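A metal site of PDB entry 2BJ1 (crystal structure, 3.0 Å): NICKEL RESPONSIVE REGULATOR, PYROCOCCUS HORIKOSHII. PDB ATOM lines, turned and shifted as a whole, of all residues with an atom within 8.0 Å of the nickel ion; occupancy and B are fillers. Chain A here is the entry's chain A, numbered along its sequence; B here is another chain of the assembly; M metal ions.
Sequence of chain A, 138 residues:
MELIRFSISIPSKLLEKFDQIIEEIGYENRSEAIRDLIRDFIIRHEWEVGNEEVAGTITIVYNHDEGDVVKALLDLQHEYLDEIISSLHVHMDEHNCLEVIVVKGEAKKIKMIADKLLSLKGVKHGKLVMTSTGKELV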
ATOM      1  N   ASN A  63      11.906 -28.406  29.445  1.00  0.00           N
ATOM      2  CA  ASN A  63      12.996 -28.133  28.516  1.00  0.00           C
ATOM      3  C   ASN A  63      12.411 -27.020  27.653  1.00  0.00           C
ATOM      4  O   ASN A  63      11.432 -27.260  26.936  1.00  0.00           O
ATOM      5  CB  ASN A  63      13.262 -29.368  27.657  1.00  0.00           C
ATOM      6  CG  ASN A  63      14.507 -29.256  26.823  1.00  0.00           C
ATOM      7  OD1 ASN A  63      14.715 -28.260  26.127  1.00  0.00           O
ATOM      8  ND2 ASN A  63      15.346 -30.279  26.878  1.00  0.00           N
ATOM      9  N   HIS A  64      12.981 -25.825  27.704  1.00  0.00           N
ATOM     10  CA  HIS A  64      12.418 -24.708  26.953  1.00  0.00           C
ATOM     11  C   HIS A  64      12.583 -24.734  25.424  1.00  0.00           C
ATOM     12  O   HIS A  64      12.168 -23.799  24.743  1.00  0.00           O
ATOM     13  CB  HIS A  64      12.948 -23.372  27.488  1.00  0.00           C
ATOM     14  CG  HIS A  64      14.385 -23.131  27.197  1.00  0.00           C
ATOM     15  ND1 HIS A  64      15.390 -23.976  27.626  1.00  0.00           N
ATOM     16  CD2 HIS A  64      15.006 -22.145  26.511  1.00  0.00           C
ATOM     17  CE1 HIS A  64      16.560 -23.509  27.230  1.00  0.00           C
ATOM     18  NE2 HIS A  64      16.353 -22.395  26.544  1.00  0.00           N
ATOM     19  N   ASP A  65      13.178 -25.796  24.895  1.00  0.00           N
ATOM     20  CA  ASP A  65      13.353 -25.901  23.450  1.00  0.00           C
ATOM     21  C   ASP A  65      12.476 -27.025  22.924  1.00  0.00           C
ATOM     22  O   ASP A  65      11.875 -26.920  21.849  1.00  0.00           O
ATOM     23  CB  ASP A  65      14.822 -26.198  23.111  1.00  0.00           C
ATOM     24  CG  ASP A  65      15.778 -25.173  23.679  1.00  0.00           C
ATOM     25  OD1 ASP A  65      15.599 -23.957  23.400  1.00  0.00           O
ATOM     26  OD2 ASP A  65      16.712 -25.568  24.403  1.00  0.00           O
ATOM     27  N   GLU A  66      12.401 -28.087  23.723  1.00  0.00           N
ATOM     28  CA  GLU A  66      11.627 -29.278  23.416  1.00  0.00           C
ATOM     29  C   GLU A  66      10.152 -29.018  23.130  1.00  0.00           C
ATOM     30  O   GLU A  66       9.283 -29.418  23.910  1.00  0.00           O
ATOM     31  CB  GLU A  66      11.769 -30.279  24.566  1.00  0.00           C
ATOM     32  CG  GLU A  66      10.995 -31.579  24.384  1.00  0.00           C
ATOM     33  CD  GLU A  66      11.167 -32.511  25.564  1.00  0.00           C
ATOM     34  OE1 GLU A  66      10.506 -33.571  25.597  1.00  0.00           O
ATOM     35  OE2 GLU A  66      11.956 -32.163  26.474  1.00  0.00           O
ATOM     36  N   VAL A  70       7.188 -23.619  26.125  1.00  0.00           N
ATOM     37  CA  VAL A  70       7.311 -22.272  26.690  1.00  0.00           C
ATOM     38  C   VAL A  70       6.156 -21.336  26.342  1.00  0.00           C
ATOM     39  O   VAL A  70       5.469 -20.816  27.231  1.00  0.00           O
ATOM     40  CB  VAL A  70       8.629 -21.605  26.267  1.00  0.00           C
ATOM     41  CG1 VAL A  70       8.640 -20.130  26.649  1.00  0.00           C
ATOM     42  CG2 VAL A  70       9.798 -22.330  26.930  1.00  0.00           C
ATOM     43  N   GLU A  94      21.509 -25.821  30.661  1.00  0.00           N
ATOM     44  CA  GLU A  94      21.369 -25.180  29.353  1.00  0.00           C
ATOM     45  C   GLU A  94      19.987 -25.285  28.694  1.00  0.00           C
ATOM     46  O   GLU A  94      19.618 -24.419  27.915  1.00  0.00           O
ATOM     47  CB  GLU A  94      22.443 -25.748  28.425  1.00  0.00           C
ATOM     48  CG  GLU A  94      22.419 -25.234  27.009  1.00  0.00           C
ATOM     49  CD  GLU A  94      23.517 -25.842  26.153  1.00  0.00           C
ATOM     50  OE1 GLU A  94      23.533 -25.608  24.927  1.00  0.00           O
ATOM     51  OE2 GLU A  94      24.386 -26.552  26.721  1.00  0.00           O
ATOM     52  N   HIS A  95      19.210 -26.326  29.013  1.00  0.00           N
ATOM     53  CA  HIS A  95      17.893 -26.485  28.374  1.00  0.00           C
ATOM     54  C   HIS A  95      16.748 -26.764  29.350  1.00  0.00           C
ATOM     55  O   HIS A  95      15.568 -26.607  28.996  1.00  0.00           O
ATOM     56  CB  HIS A  95      17.945 -27.629  27.350  1.00  0.00           C
ATOM     57  CG  HIS A  95      18.984 -27.470  26.301  1.00  0.00           C
ATOM     58  ND1 HIS A  95      18.923 -26.487  25.327  1.00  0.00           N
ATOM     59  CD2 HIS A  95      20.120 -28.166  26.051  1.00  0.00           C
ATOM     60  CE1 HIS A  95      19.971 -26.586  24.529  1.00  0.00           C
ATOM     61  NE2 HIS A  95      20.714 -27.594  24.953  1.00  0.00           N
ATOM     62  N   ASN A  96      17.079 -27.188  30.560  1.00  0.00           N
ATOM     63  CA  ASN A  96      16.055 -27.509  31.528  1.00  0.00           C
ATOM     64  C   ASN A  96      15.699 -26.449  32.581  1.00  0.00           C
ATOM     65  O   ASN A  96      16.585 -25.839  33.210  1.00  0.00           O
ATOM     66  CB  ASN A  96      16.388 -28.852  32.186  1.00  0.00           C
ATOM     67  CG  ASN A  96      16.137 -30.011  31.243  1.00  0.00           C
ATOM     68  OD1 ASN A  96      14.983 -30.318  30.925  1.00  0.00           O
ATOM     69  ND2 ASN A  96      17.199 -30.646  30.783  1.00  0.00           N
ATOM     70  N   LYS B  71      11.111 -16.447  23.624  1.00  0.00           N
ATOM     71  CA  LYS B  71      12.139 -17.387  23.223  1.00  0.00           C
ATOM     72  C   LYS B  71      13.482 -16.754  23.569  1.00  0.00           C
ATOM     73  O   LYS B  71      14.219 -17.245  24.420  1.00  0.00           O
ATOM     74  CB  LYS B  71      12.021 -17.617  21.713  1.00  0.00           C
ATOM     75  CG  LYS B  71      12.871 -18.720  21.123  1.00  0.00           C
ATOM     76  CD  LYS B  71      12.610 -18.816  19.617  1.00  0.00           C
ATOM     77  CE  LYS B  71      13.233 -20.068  19.005  1.00  0.00           C
ATOM     78  NZ  LYS B  71      14.717 -20.100  19.163  1.00  0.00           N
ATOM     79  N   ALA B  72      13.762 -15.629  22.913  1.00  0.00           N
ATOM     80  CA  ALA B  72      15.013 -14.894  23.112  1.00  0.00           C
ATOM     81  C   ALA B  72      15.409 -14.728  24.565  1.00  0.00           C
ATOM     82  O   ALA B  72      16.558 -14.956  24.931  1.00  0.00           O
ATOM     83  CB  ALA B  72      14.907 -13.538  22.442  1.00  0.00           C
ATOM     84  N   LEU B  73      14.447 -14.321  25.394  1.00  0.00           N
ATOM     85  CA  LEU B  73      14.688 -14.105  26.814  1.00  0.00           C
ATOM     86  C   LEU B  73      15.292 -15.327  27.477  1.00  0.00           C
ATOM     87  O   LEU B  73      16.294 -15.219  28.167  1.00  0.00           O
ATOM     88  CB  LEU B  73      13.402 -13.713  27.528  1.00  0.00           C
ATOM     89  CG  LEU B  73      13.028 -12.224  27.469  1.00  0.00           C
ATOM     90  CD1 LEU B  73      11.689 -11.973  28.144  1.00  0.00           C
ATOM     91  CD2 LEU B  73      14.109 -11.425  28.164  1.00  0.00           C
ATOM     92  N   LEU B  74      14.674 -16.487  27.285  1.00  0.00           N
ATOM     93  CA  LEU B  74      15.186 -17.697  27.910  1.00  0.00           C
ATOM     94  C   LEU B  74      16.558 -18.093  27.378  1.00  0.00           C
ATOM     95  O   LEU B  74      17.484 -18.327  28.161  1.00  0.00           O
ATOM     96  CB  LEU B  74      14.187 -18.841  27.713  1.00  0.00           C
ATOM     97  CG  LEU B  74      12.913 -18.680  28.544  1.00  0.00           C
ATOM     98  CD1 LEU B  74      11.838 -19.617  28.034  1.00  0.00           C
ATOM     99  CD2 LEU B  74      13.221 -18.963  30.007  1.00  0.00           C
ATOM    100  N   ASP B  75      16.681 -18.149  26.059  1.00  0.00           N
ATOM    101  CA  ASP B  75      17.937 -18.515  25.424  1.00  0.00           C
ATOM    102  C   ASP B  75      19.071 -17.651  25.940  1.00  0.00           C
ATOM    103  O   ASP B  75      20.144 -18.155  26.287  1.00  0.00           O
ATOM    104  CB  ASP B  75      17.799 -18.373  23.914  1.00  0.00           C
ATOM    105  CG  ASP B  75      16.517 -18.985  23.380  1.00  0.00           C
ATOM    106  OD1 ASP B  75      16.236 -20.171  23.688  1.00  0.00           O
ATOM    107  OD2 ASP B  75      15.779 -18.289  22.659  1.00  0.00           O
ATOM    108  N   LEU B  76      18.804 -16.352  26.009  1.00  0.00           N
ATOM    109  CA  LEU B  76      19.771 -15.364  26.493  1.00  0.00           C
ATOM    110  C   LEU B  76      20.058 -15.617  27.981  1.00  0.00           C
ATOM    111  O   LEU B  76      21.214 -15.573  28.405  1.00  0.00           O
ATOM    112  CB  LEU B  76      19.204 -13.946  26.324  1.00  0.00           C
ATOM    113  CG  LEU B  76      20.163 -12.755  26.083  1.00  0.00           C
ATOM    114  CD1 LEU B  76      19.386 -11.446  26.213  1.00  0.00           C
ATOM    115  CD2 LEU B  76      21.318 -12.786  27.061  1.00  0.00           C
ATOM    116  N   GLN B  77      19.010 -15.881  28.758  1.00  0.00           N
ATOM    117  CA  GLN B  77      19.172 -16.135  30.183  1.00  0.00           C
ATOM    118  C   GLN B  77      19.889 -17.433  30.472  1.00  0.00           C
ATOM    119  O   GLN B  77      20.752 -17.493  31.347  1.00  0.00           O
ATOM    120  CB  GLN B  77      17.819 -16.127  30.887  1.00  0.00           C
ATOM    121  CG  GLN B  77      17.143 -14.784  30.936  1.00  0.00           C
ATOM    122  CD  GLN B  77      15.978 -14.740  31.906  1.00  0.00           C
ATOM    123  OE1 GLN B  77      16.158 -14.946  33.107  1.00  0.00           O
ATOM    124  NE2 GLN B  77      14.786 -14.468  31.384  1.00  0.00           N
ATOM    125  N   HIS B  78      19.548 -18.493  29.749  1.00  0.00           N
ATOM    126  CA  HIS B  78      20.198 -19.772  29.976  1.00  0.00           C
ATOM    127  C   HIS B  78      21.651 -19.714  29.516  1.00  0.00           C
ATOM    128  O   HIS B  78      22.463 -20.559  29.888  1.00  0.00           O
ATOM    129  CB  HIS B  78      19.415 -20.887  29.283  1.00  0.00           C
ATOM    130  CG  HIS B  78      18.348 -21.503  30.131  1.00  0.00           C
ATOM    131  ND1 HIS B  78      18.624 -22.324  31.207  1.00  0.00           N
ATOM    132  CD2 HIS B  78      16.989 -21.403  30.079  1.00  0.00           C
ATOM    133  CE1 HIS B  78      17.491 -22.696  31.772  1.00  0.00           C
ATOM    134  NE2 HIS B  78      16.492 -22.157  31.116  1.00  0.00           N
ATOM    135  N   GLU B  79      21.972 -18.694  28.720  1.00  0.00           N
ATOM    136  CA  GLU B  79      23.329 -18.500  28.219  1.00  0.00           C
ATOM    137  C   GLU B  79      24.208 -17.963  29.329  1.00  0.00           C
ATOM    138  O   GLU B  79      25.433 -18.110  29.291  1.00  0.00           O
ATOM    139  CB  GLU B  79      23.325 -17.511  27.051  1.00  0.00           C
ATOM    140  CG  GLU B  79      24.718 -17.089  26.597  1.00  0.00           C
ATOM    141  CD  GLU B  79      24.714 -15.840  25.742  1.00  0.00           C
ATOM    142  OE1 GLU B  79      25.809 -15.302  25.467  1.00  0.00           O
ATOM    143  OE2 GLU B  79      23.619 -15.379  25.356  1.00  0.00           O
HETATM  144 NI    NI M   1      17.287 -22.343  24.418  1.00  0.00          NI
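The nickel ion is bound by NE2 of His 64 (2.3 Å), OD1 of Asp 75 of chain B (2.5 Å) and OD1 of Asp 65 (2.5 Å).
The nickel ion has three donor atoms within binding distance.
Along chain A the residues within 4 Å of the nickel ion span positions 64 to 65.
The nearest printed residue that does not touch the nickel ion is His 95 (4.5 Å).
O of His 95 sits at hydrogen-bond distance from ND1 of His 64 (3.0 Å).
N of Asp 65 lies close to OD1 of Asn 63 (3.2 Å).
The side-chain carboxylate (OD2) of Asp 75 of chain B lies close to the backbone carbonyl oxygen (O) of Lys 71 of chain B, at 2.6 Å.
OD2 of Asp 65 lies within hydrogen-bond range of ND1 of His 95, 2.6 Å away.
OD2 of Asp 75 of chain B is in hydrogen-bond range of N of Ala 72 of chain B, at 3.3 Å.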
